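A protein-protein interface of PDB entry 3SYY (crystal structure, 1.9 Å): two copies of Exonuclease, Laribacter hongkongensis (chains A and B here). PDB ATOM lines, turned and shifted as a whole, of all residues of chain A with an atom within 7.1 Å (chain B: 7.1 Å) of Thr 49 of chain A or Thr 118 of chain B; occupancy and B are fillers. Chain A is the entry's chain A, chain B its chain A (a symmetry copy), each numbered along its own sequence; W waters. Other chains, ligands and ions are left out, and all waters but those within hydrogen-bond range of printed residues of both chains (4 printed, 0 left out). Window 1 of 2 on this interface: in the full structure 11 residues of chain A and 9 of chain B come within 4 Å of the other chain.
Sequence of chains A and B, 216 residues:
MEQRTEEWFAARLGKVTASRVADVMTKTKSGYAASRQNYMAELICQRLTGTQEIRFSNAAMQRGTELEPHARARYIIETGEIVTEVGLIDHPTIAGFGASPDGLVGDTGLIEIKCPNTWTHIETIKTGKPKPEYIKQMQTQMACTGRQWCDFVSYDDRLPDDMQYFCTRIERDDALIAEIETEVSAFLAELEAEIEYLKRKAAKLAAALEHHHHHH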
ATOM      1  N   LEU A  13      -7.517  27.286   2.637  1.00  0.00           N
ATOM      2  CA  LEU A  13      -8.385  26.398   3.455  1.00  0.00           C
ATOM      3  C   LEU A  13      -9.203  27.127   4.527  1.00  0.00           C
ATOM      4  O   LEU A  13      -8.664  27.877   5.326  1.00  0.00           O
ATOM      5  CB  LEU A  13      -7.577  25.242   4.091  1.00  0.00           C
ATOM      6  CG  LEU A  13      -8.435  24.172   4.814  1.00  0.00           C
ATOM      7  CD1 LEU A  13      -9.077  23.266   3.822  1.00  0.00           C
ATOM      8  CD2 LEU A  13      -7.550  23.350   5.787  1.00  0.00           C
ATOM      9  N   ALA A  41     -21.507  25.985   4.041  1.00  0.00           N
ATOM     10  CA  ALA A  41     -21.336  24.552   4.264  1.00  0.00           C
ATOM     11  C   ALA A  41     -19.968  24.102   3.771  1.00  0.00           C
ATOM     12  O   ALA A  41     -19.261  23.329   4.436  1.00  0.00           O
ATOM     13  CB  ALA A  41     -22.490  23.754   3.582  1.00  0.00           C
ATOM     14  N   GLU A  42     -19.535  24.618   2.614  1.00  0.00           N
ATOM     15  CA  GLU A  42     -18.236  24.253   2.106  1.00  0.00           C
ATOM     16  C   GLU A  42     -17.121  24.657   3.080  1.00  0.00           C
ATOM     17  O   GLU A  42     -16.158  23.903   3.298  1.00  0.00           O
ATOM     18  CB  GLU A  42     -17.933  25.023   0.792  1.00  0.00           C
ATOM     19  CG  GLU A  42     -18.250  24.357  -0.503  1.00  0.00           C
ATOM     20  CD  GLU A  42     -17.966  25.330  -1.667  1.00  0.00           C
ATOM     21  OE1 GLU A  42     -18.939  25.849  -2.231  1.00  0.00           O
ATOM     22  OE2 GLU A  42     -16.780  25.586  -1.922  1.00  0.00           O
ATOM     23  N   LEU A  43     -17.192  25.884   3.584  1.00  0.00           N
ATOM     24  CA  LEU A  43     -16.127  26.373   4.481  1.00  0.00           C
ATOM     25  C   LEU A  43     -16.183  25.651   5.870  1.00  0.00           C
ATOM     26  O   LEU A  43     -15.143  25.364   6.470  1.00  0.00           O
ATOM     27  CB  LEU A  43     -16.262  27.870   4.640  1.00  0.00           C
ATOM     28  CG  LEU A  43     -16.041  28.649   3.326  1.00  0.00           C
ATOM     29  CD1 LEU A  43     -15.909  30.136   3.655  1.00  0.00           C
ATOM     30  CD2 LEU A  43     -14.801  28.182   2.679  1.00  0.00           C
ATOM     31  N   ILE A  44     -17.387  25.346   6.343  1.00  0.00           N
ATOM     32  CA  ILE A  44     -17.525  24.546   7.606  1.00  0.00           C
ATOM     33  C   ILE A  44     -16.808  23.218   7.465  1.00  0.00           C
ATOM     34  O   ILE A  44     -15.954  22.859   8.303  1.00  0.00           O
ATOM     35  CB  ILE A  44     -18.988  24.351   8.015  1.00  0.00           C
ATOM     36  CG1 ILE A  44     -19.549  25.695   8.452  1.00  0.00           C
ATOM     37  CG2 ILE A  44     -19.108  23.264   9.157  1.00  0.00           C
ATOM     38  CD1 ILE A  44     -21.072  25.762   8.501  1.00  0.00           C
ATOM     39  N   CYS A  45     -17.095  22.498   6.376  1.00  0.00           N
ATOM     40  CA  CYS A  45     -16.471  21.212   6.173  1.00  0.00           C
ATOM     41  C   CYS A  45     -14.942  21.326   6.003  1.00  0.00           C
ATOM     42  O   CYS A  45     -14.204  20.469   6.450  1.00  0.00           O
ATOM     43  CB  CYS A  45     -17.136  20.425   5.004  1.00  0.00           C
ATOM     44  SG  CYS A  45     -18.920  20.202   5.296  1.00  0.00           S
ATOM     45  N   GLN A  46     -14.457  22.369   5.313  1.00  0.00           N
ATOM     46  CA  GLN A  46     -13.012  22.554   5.206  1.00  0.00           C
ATOM     47  C   GLN A  46     -12.356  22.745   6.584  1.00  0.00           C
ATOM     48  O   GLN A  46     -11.356  22.148   6.862  1.00  0.00           O
ATOM     49  CB  GLN A  46     -12.680  23.777   4.318  1.00  0.00           C
ATOM     50  CG  GLN A  46     -12.927  23.496   2.826  1.00  0.00           C
ATOM     51  CD  GLN A  46     -12.589  24.690   1.902  1.00  0.00           C
ATOM     52  OE1 GLN A  46     -11.919  25.630   2.295  1.00  0.00           O
ATOM     53  NE2 GLN A  46     -13.124  24.657   0.698  1.00  0.00           N
ATOM     54  N   ARG A  47     -12.943  23.584   7.414  1.00  0.00           N
ATOM     55  CA  ARG A  47     -12.368  23.878   8.730  1.00  0.00           C
ATOM     56  C   ARG A  47     -12.423  22.645   9.636  1.00  0.00           C
ATOM     57  O   ARG A  47     -11.460  22.349  10.318  1.00  0.00           O
ATOM     58  CB  ARG A  47     -13.064  25.062   9.361  1.00  0.00           C
ATOM     59  CG  ARG A  47     -12.624  26.361   8.697  1.00  0.00           C
ATOM     60  CD  ARG A  47     -13.211  27.549   9.438  1.00  0.00           C
ATOM     61  NE  ARG A  47     -12.958  28.823   8.753  1.00  0.00           N
ATOM     62  CZ  ARG A  47     -12.843  29.994   9.370  1.00  0.00           C
ATOM     63  NH1 ARG A  47     -12.960  30.081  10.705  1.00  0.00           N
ATOM     64  NH2 ARG A  47     -12.654  31.097   8.647  1.00  0.00           N
ATOM     65  N   LEU A  48     -13.524  21.911   9.599  1.00  0.00           N
ATOM     66  CA  LEU A  48     -13.679  20.706  10.438  1.00  0.00           C
ATOM     67  C   LEU A  48     -12.830  19.544  10.000  1.00  0.00           C
ATOM     68  O   LEU A  48     -12.191  18.881  10.855  1.00  0.00           O
ATOM     69  CB  LEU A  48     -15.158  20.279  10.482  1.00  0.00           C
ATOM     70  CG  LEU A  48     -16.037  21.147  11.364  1.00  0.00           C
ATOM     71  CD1 LEU A  48     -17.529  20.737  11.165  1.00  0.00           C
ATOM     72  CD2 LEU A  48     -15.575  21.052  12.887  1.00  0.00           C
ATOM     73  N   THR A  49     -12.786  19.288   8.682  1.00  0.00           N
ATOM     74  CA  THR A  49     -12.041  18.133   8.156  1.00  0.00           C
ATOM     75  C   THR A  49     -10.569  18.424   7.864  1.00  0.00           C
ATOM     76  O   THR A  49      -9.726  17.491   7.762  1.00  0.00           O
ATOM     77  CB  THR A  49     -12.640  17.628   6.828  1.00  0.00           C
ATOM     78  OG1 THR A  49     -12.487  18.655   5.821  1.00  0.00           O
ATOM     79  CG2 THR A  49     -14.094  17.288   7.006  1.00  0.00           C
ATOM     80  N   GLY A  50     -10.238  19.707   7.734  1.00  0.00           N
ATOM     81  CA  GLY A  50      -8.872  20.060   7.391  1.00  0.00           C
ATOM     82  C   GLY A  50      -8.481  19.793   5.944  1.00  0.00           C
ATOM     83  O   GLY A  50      -7.318  19.883   5.619  1.00  0.00           O
ATOM     84  N   THR A  51      -9.432  19.456   5.083  1.00  0.00           N
ATOM     85  CA  THR A  51      -9.179  19.300   3.638  1.00  0.00           C
ATOM     86  C   THR A  51     -10.344  19.861   2.825  1.00  0.00           C
ATOM     87  O   THR A  51     -11.455  20.024   3.341  1.00  0.00           O
ATOM     88  CB  THR A  51      -9.000  17.841   3.179  1.00  0.00           C
ATOM     89  OG1 THR A  51     -10.081  17.030   3.682  1.00  0.00           O
ATOM     90  CG2 THR A  51      -7.634  17.267   3.600  1.00  0.00           C
ATOM     91  N   GLN A  52     -10.069  20.188   1.559  1.00  0.00           N
ATOM     92  CA  GLN A  52     -11.112  20.641   0.641  1.00  0.00           C
ATOM     93  C   GLN A  52     -11.491  19.497  -0.285  1.00  0.00           C
ATOM     94  O   GLN A  52     -10.665  18.615  -0.527  1.00  0.00           O
ATOM     95  CB  GLN A  52     -10.696  21.901  -0.162  1.00  0.00           C
ATOM     96  CG  GLN A  52      -9.318  21.907  -0.793  1.00  0.00           C
ATOM     97  CD  GLN A  52      -8.243  22.577   0.093  1.00  0.00           C
ATOM     98  OE1 GLN A  52      -7.319  21.904   0.571  1.00  0.00           O
ATOM     99  NE2 GLN A  52      -8.354  23.917   0.298  1.00  0.00           N
ATOM    100  N   GLU A  53     -12.731  19.510  -0.788  1.00  0.00           N
ATOM    101  CA  GLU A  53     -13.185  18.554  -1.822  1.00  0.00           C
ATOM    102  C   GLU A  53     -12.552  18.850  -3.195  1.00  0.00           C
ATOM    103  O   GLU A  53     -12.401  20.017  -3.560  1.00  0.00           O
ATOM    104  CB  GLU A  53     -14.712  18.574  -1.940  1.00  0.00           C
ATOM    105  CG  GLU A  53     -15.428  18.027  -0.702  1.00  0.00           C
ATOM    106  CD  GLU A  53     -15.036  16.581  -0.384  1.00  0.00           C
ATOM    107  OE1 GLU A  53     -14.915  15.778  -1.343  1.00  0.00           O
ATOM    108  OE2 GLU A  53     -14.854  16.247   0.820  1.00  0.00           O
ATOM    109  N   ARG B  63     -16.333   6.675  -3.319  1.00  0.00           N
ATOM    110  CA  ARG B  63     -15.598   6.867  -2.069  1.00  0.00           C
ATOM    111  C   ARG B  63     -16.464   6.288  -0.937  1.00  0.00           C
ATOM    112  O   ARG B  63     -15.979   5.517  -0.103  1.00  0.00           O
ATOM    113  CB  ARG B  63     -15.310   8.352  -1.832  1.00  0.00           C
ATOM    114  CG  ARG B  63     -14.494   8.603  -0.556  1.00  0.00           C
ATOM    115  CD  ARG B  63     -14.896   9.917   0.068  1.00  0.00           C
ATOM    116  NE  ARG B  63     -14.650   9.875   1.505  1.00  0.00           N
ATOM    117  CZ  ARG B  63     -15.563   9.548   2.423  1.00  0.00           C
ATOM    118  NH1 ARG B  63     -15.188   9.548   3.694  1.00  0.00           N
ATOM    119  NH2 ARG B  63     -16.829   9.248   2.078  1.00  0.00           N
ATOM    120  N   CYS B 115     -22.455   6.550   3.796  1.00  0.00           N
ATOM    121  CA  CYS B 115     -21.178   7.252   3.864  1.00  0.00           C
ATOM    122  C   CYS B 115     -21.193   8.401   2.850  1.00  0.00           C
ATOM    123  O   CYS B 115     -20.598   8.271   1.777  1.00  0.00           O
ATOM    124  CB  CYS B 115     -20.033   6.314   3.517  1.00  0.00           C
ATOM    125  SG  CYS B 115     -19.810   4.928   4.798  1.00  0.00           S
ATOM    126  N   PRO B 116     -21.841   9.507   3.206  1.00  0.00           N
ATOM    127  CA  PRO B 116     -22.164  10.509   2.281  1.00  0.00           C
ATOM    128  C   PRO B 116     -21.154  11.644   2.296  1.00  0.00           C
ATOM    129  O   PRO B 116     -20.074  11.535   2.922  1.00  0.00           O
ATOM    130  CB  PRO B 116     -23.510  10.983   2.816  1.00  0.00           C
ATOM    131  CG  PRO B 116     -23.196  11.073   4.353  1.00  0.00           C
ATOM    132  CD  PRO B 116     -22.439   9.763   4.537  1.00  0.00           C
ATOM    133  N   ASN B 117     -21.525  12.745   1.629  1.00  0.00           N
ATOM    134  CA  ASN B 117     -20.710  13.961   1.678  1.00  0.00           C
ATOM    135  C   ASN B 117     -20.702  14.469   3.111  1.00  0.00           C
ATOM    136  O   ASN B 117     -21.632  14.246   3.865  1.00  0.00           O
ATOM    137  CB  ASN B 117     -21.310  15.052   0.786  1.00  0.00           C
ATOM    138  CG  ASN B 117     -20.984  14.842  -0.685  1.00  0.00           C
ATOM    139  OD1 ASN B 117     -20.078  14.063  -1.047  1.00  0.00           O
ATOM    140  ND2 ASN B 117     -21.733  15.534  -1.555  1.00  0.00           N
ATOM    141  N   THR B 118     -19.671  15.219   3.461  1.00  0.00           N
ATOM    142  CA  THR B 118     -19.467  15.604   4.863  1.00  0.00           C
ATOM    143  C   THR B 118     -20.622  16.398   5.338  1.00  0.00           C
ATOM    144  O   THR B 118     -21.108  16.165   6.437  1.00  0.00           O
ATOM    145  CB  THR B 118     -18.170  16.403   4.998  1.00  0.00           C
ATOM    146  OG1 THR B 118     -17.122  15.521   4.621  1.00  0.00           O
ATOM    147  CG2 THR B 118     -17.949  16.846   6.469  1.00  0.00           C
ATOM    148  N   TRP B 119     -21.071  17.367   4.525  1.00  0.00           N
ATOM    149  CA  TRP B 119     -22.206  18.204   4.946  1.00  0.00           C
ATOM    150  C   TRP B 119     -23.522  17.434   5.159  1.00  0.00           C
ATOM    151  O   TRP B 119     -24.309  17.755   6.058  1.00  0.00           O
ATOM    152  CB  TRP B 119     -22.426  19.397   3.994  1.00  0.00           C
ATOM    153  CG  TRP B 119     -23.432  20.368   4.551  1.00  0.00           C
ATOM    154  CD1 TRP B 119     -24.667  20.666   4.035  1.00  0.00           C
ATOM    155  CD2 TRP B 119     -23.281  21.177   5.728  1.00  0.00           C
ATOM    156  NE1 TRP B 119     -25.288  21.611   4.829  1.00  0.00           N
ATOM    157  CE2 TRP B 119     -24.468  21.921   5.882  1.00  0.00           C
ATOM    158  CE3 TRP B 119     -22.261  21.326   6.679  1.00  0.00           C
ATOM    159  CZ2 TRP B 119     -24.658  22.844   6.945  1.00  0.00           C
ATOM    160  CZ3 TRP B 119     -22.447  22.246   7.755  1.00  0.00           C
ATOM    161  CH2 TRP B 119     -23.650  22.977   7.871  1.00  0.00           C
ATOM    162  N   THR B 120     -23.769  16.429   4.318  1.00  0.00           N
ATOM    163  CA  THR B 120     -24.963  15.598   4.501  1.00  0.00           C
ATOM    164  C   THR B 120     -24.868  14.869   5.860  1.00  0.00           C
ATOM    165  O   THR B 120     -25.843  14.784   6.611  1.00  0.00           O
ATOM    166  CB  THR B 120     -25.042  14.568   3.371  1.00  0.00           C
ATOM    167  OG1 THR B 120     -25.130  15.297   2.133  1.00  0.00           O
ATOM    168  CG2 THR B 120     -26.304  13.648   3.512  1.00  0.00           C
ATOM    169  N   HIS B 121     -23.677  14.405   6.170  1.00  0.00           N
ATOM    170  CA  HIS B 121     -23.449  13.696   7.457  1.00  0.00           C
ATOM    171  C   HIS B 121     -23.725  14.658   8.626  1.00  0.00           C
ATOM    172  O   HIS B 121     -24.452  14.318   9.606  1.00  0.00           O
ATOM    173  CB  HIS B 121     -22.016  13.189   7.481  1.00  0.00           C
ATOM    174  CG  HIS B 121     -21.677  12.421   8.729  1.00  0.00           C
ATOM    175  ND1 HIS B 121     -20.933  12.954   9.767  1.00  0.00           N
ATOM    176  CD2 HIS B 121     -22.049  11.179   9.122  1.00  0.00           C
ATOM    177  CE1 HIS B 121     -20.810  12.045  10.727  1.00  0.00           C
ATOM    178  NE2 HIS B 121     -21.483  10.956  10.361  1.00  0.00           N
ATOM    179  N   ILE B 122     -23.177  15.882   8.501  1.00  0.00           N
ATOM    180  CA  ILE B 122     -23.372  16.942   9.497  1.00  0.00           C
ATOM    181  C   ILE B 122     -24.837  17.290   9.655  1.00  0.00           C
ATOM    182  O   ILE B 122     -25.352  17.459  10.786  1.00  0.00           O
ATOM    183  CB  ILE B 122     -22.509  18.210   9.170  1.00  0.00           C
ATOM    184  CG1 ILE B 122     -21.041  17.821   9.375  1.00  0.00           C
ATOM    185  CG2 ILE B 122     -22.962  19.420  10.024  1.00  0.00           C
ATOM    186  CD1 ILE B 122     -19.996  18.877   8.924  1.00  0.00           C
ATOM    187  N   GLU B 123     -25.560  17.373   8.531  1.00  0.00           N
ATOM    188  CA  GLU B 123     -26.968  17.674   8.662  1.00  0.00           C
ATOM    189  C   GLU B 123     -27.710  16.532   9.346  1.00  0.00           C
ATOM    190  O   GLU B 123     -28.674  16.796  10.048  1.00  0.00           O
ATOM    191  CB  GLU B 123     -27.613  17.995   7.307  1.00  0.00           C
ATOM    192  CG  GLU B 123     -27.201  19.396   6.830  1.00  0.00           C
ATOM    193  CD  GLU B 123     -27.954  19.834   5.552  1.00  0.00           C
ATOM    194  OE1 GLU B 123     -28.110  18.989   4.627  1.00  0.00           O
ATOM    195  OE2 GLU B 123     -28.352  21.020   5.489  1.00  0.00           O
ATOM    196  N   THR B 124     -27.280  15.293   9.141  1.00  0.00           N
ATOM    197  CA  THR B 124     -27.906  14.141   9.852  1.00  0.00           C
ATOM    198  C   THR B 124     -27.655  14.285  11.376  1.00  0.00           C
ATOM    199  O   THR B 124     -28.586  14.106  12.174  1.00  0.00           O
ATOM    200  CB  THR B 124     -27.373  12.806   9.357  1.00  0.00           C
ATOM    201  OG1 THR B 124     -27.707  12.702   7.967  1.00  0.00           O
ATOM    202  CG2 THR B 124     -28.021  11.594  10.129  1.00  0.00           C
ATOM    203  N   ASP B 156     -18.519   9.371   8.543  1.00  0.00           N
ATOM    204  CA  ASP B 156     -17.545  10.117   7.743  1.00  0.00           C
ATOM    205  C   ASP B 156     -16.236  10.253   8.503  1.00  0.00           C
ATOM    206  O   ASP B 156     -16.151  11.032   9.447  1.00  0.00           O
ATOM    207  CB  ASP B 156     -18.103  11.508   7.420  1.00  0.00           C
ATOM    208  CG  ASP B 156     -17.223  12.264   6.389  1.00  0.00           C
ATOM    209  OD1 ASP B 156     -16.103  11.815   6.070  1.00  0.00           O
ATOM    210  OD2 ASP B 156     -17.692  13.271   5.885  1.00  0.00           O
ATOM    211  N   ASP B 157     -15.222   9.547   8.031  1.00  0.00           N
ATOM    212  CA  ASP B 157     -13.939   9.569   8.669  1.00  0.00           C
ATOM    213  C   ASP B 157     -13.129  10.842   8.438  1.00  0.00           C
ATOM    214  O   ASP B 157     -12.037  10.977   9.001  1.00  0.00           O
ATOM    215  CB  ASP B 157     -13.130   8.342   8.232  1.00  0.00           C
ATOM    216  CG  ASP B 157     -12.716   8.406   6.778  1.00  0.00           C
ATOM    217  OD1 ASP B 157     -11.772   7.724   6.425  1.00  0.00           O
ATOM    218  OD2 ASP B 157     -13.303   9.140   5.965  1.00  0.00           O
ATOM    219  N   ARG B 158     -13.625  11.772   7.626  1.00  0.00           N
ATOM    220  CA  ARG B 158     -12.843  13.020   7.416  1.00  0.00           C
ATOM    221  C   ARG B 158     -12.954  13.973   8.587  1.00  0.00           C
ATOM    222  O   ARG B 158     -12.158  14.907   8.695  1.00  0.00           O
ATOM    223  CB  ARG B 158     -13.292  13.726   6.133  1.00  0.00           C
ATOM    224  CG  ARG B 158     -12.971  12.873   4.918  1.00  0.00           C
ATOM    225  CD  ARG B 158     -13.715  13.352   3.649  1.00  0.00           C
ATOM    226  NE  ARG B 158     -15.115  12.967   3.728  1.00  0.00           N
ATOM    227  CZ  ARG B 158     -15.936  12.908   2.681  1.00  0.00           C
ATOM    228  NH1 ARG B 158     -15.460  13.182   1.455  1.00  0.00           N
ATOM    229  NH2 ARG B 158     -17.206  12.537   2.857  1.00  0.00           N
ATOM    230  N   LEU B 159     -13.959  13.750   9.444  1.00  0.00           N
ATOM    231  CA  LEU B 159     -14.317  14.666  10.509  1.00  0.00           C
ATOM    232  C   LEU B 159     -13.512  14.353  11.782  1.00  0.00           C
ATOM    233  O   LEU B 159     -12.923  13.303  11.860  1.00  0.00           O
ATOM    234  CB  LEU B 159     -15.811  14.541  10.786  1.00  0.00           C
ATOM    235  CG  LEU B 159     -16.662  15.251   9.716  1.00  0.00           C
ATOM    236  CD1 LEU B 159     -18.077  14.910   9.873  1.00  0.00           C
ATOM    237  CD2 LEU B 159     -16.518  16.779   9.840  1.00  0.00           C
ATOM    238  N   PRO B 160     -13.514  15.261  12.784  1.00  0.00           N
ATOM    239  CA  PRO B 160     -12.915  14.917  14.099  1.00  0.00           C
ATOM    240  C   PRO B 160     -13.592  13.656  14.658  1.00  0.00           C
ATOM    241  O   PRO B 160     -14.756  13.397  14.335  1.00  0.00           O
ATOM    242  CB  PRO B 160     -13.337  16.103  14.971  1.00  0.00           C
ATOM    243  CG  PRO B 160     -13.386  17.253  13.991  1.00  0.00           C
ATOM    244  CD  PRO B 160     -14.113  16.598  12.810  1.00  0.00           C
HETATM  245  O   HOH W   1     -10.583  16.557  11.183  1.00  0.00           O
HETATM  246  O   HOH W   2     -17.672  15.882   1.220  1.00  0.00           O
HETATM  247  O   HOH W   3      -9.695  15.112   9.063  1.00  0.00           O
HETATM  248  O   HOH W   4     -15.305  16.858   3.125  1.00  0.00           O
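NH1 of Arg 158 of chain B is in salt-bridge range of OE2 of Glu 53 of chain A (3.2 Å).
SG of Cys 45 of chain A lies within hydrogen-bond range of N of Trp 119 of chain B, 3.6 Å away.
Of chain B, only Thr 118, Arg 158 and Leu 159 come within 4 Å of Thr 49 of chain A.
Of the printed residues of chain A, Thr 118 of chain B touches Cys 45 and Thr 49.
Printed residues of chain B within 4 Å of Leu 48 of chain A: Ile 122 (3.8 Å), Leu 159 (3.8 Å) and Pro 160 (3.6 Å).
Of the printed residues of chain A, Trp 119 of chain B touches Ala 41, Ile 44 and Cys 45.
Printed residues of chain B within 4 Å of Cys 45 of chain A: Thr 118 (3.7 Å) and Trp 119 (3.6 Å).
The nearest residue of chain B that does not touch Thr 49 of chain A is Pro 160 of chain B (5.1 Å).
The nearest residue of chain A that does not touch Thr 118 of chain B is Glu 53 of chain A (4.5 Å).
The nearest printed residue of chain B that does not touch Ile 44 of chain A is Ile 122 of chain B (4.5 Å).
The guanidinium group (NH2) of Arg 158 of chain B sits at hydrogen-bond distance from the backbone carbonyl oxygen (O) of Pro 116 of chain B (3.0 Å).
The side-chain carboxylate (OD1) of Asp 156 of chain B lies within salt-bridge range of the guanidinium group (NE) of Arg 158 of chain B, at 2.8 Å.
The side-chain hydroxyl of Thr 118 of chain B is in hydrogen-bond range of the side-chain carboxylate of Asp 156 of chain B, at 2.6 Å.
NE of Arg 158 of chain B sits at hydrogen-bond distance from OG1 of Thr 118 of chain B (3.4 Å).
The side-chain hydroxyl (OG1) of Thr 49 of chain A is in hydrogen-bond range of the backbone carbonyl oxygen (O) of Thr 51 of chain A, 3.0 Å away.
The backbone carbonyl oxygen (O) of Ala 41 of chain A lies within hydrogen-bond range of the side-chain sulfur (SG) of Cys 45 of chain A, 3.3 Å away.
Ala 41 of chain A touches Trp 119 of chain B.
Ile 44 of chain A touches Trp 119 of chain B (CG2 to CZ3, 3.8 Å).
CG2 of Thr 118 of chain B touches SG of Cys 45 of chain A, 3.7 Å away.
Leu 48 of chain A touches Ile 122 of chain B.
CB of Leu 48 of chain A touches CD2 of Leu 159 of chain B, 3.8 Å away.
Pro 160 of chain B touches Leu 48 of chain A (CD to O, 3.6 Å).
Thr 118 of chain B touches Thr 49 of chain A (CG2 to CG2, 3.9 Å).
Thr 49 of chain A touches Arg 158 of chain B (CA to O, 3.3 Å).
CG2 of Thr 49 of chain A touches CD2 of Leu 159 of chain B (3.8 Å).
No position is printed for both chains.
Of the 11 pairs that touch across the chains among the printed residues, none has its exchanged pair printed and touching as well.
Of the 14 printed residues of chain A, 6 touch a printed residue of chain B.
Hydrophobic or aromatic side chains of chain A within 4 Å of the printed part of chain B: Ala 41, Ile 44 and Leu 48.
Water W4 bridges the side-chain carboxylate of Glu 53 of chain A and the side-chain hydroxyl of Thr 118 of chain B.
Water W3 bridges O of Arg 158 of chain B (2.5 Å) and O of Thr 49 of chain A (2.7 Å).
Water W1 lies within hydrogen-bond range of the backbone carbonyl oxygen (O) of Leu 48 of chain A and the backbone carbonyl oxygen (O) of Arg 158 of chain B.
Water W2 lies within hydrogen-bond range of OE2 of Glu 53 of chain A (2.9 Å), N of Thr 118 of chain B (3.1 Å) and NH1 of Arg 158 of chain B (3.5 Å).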
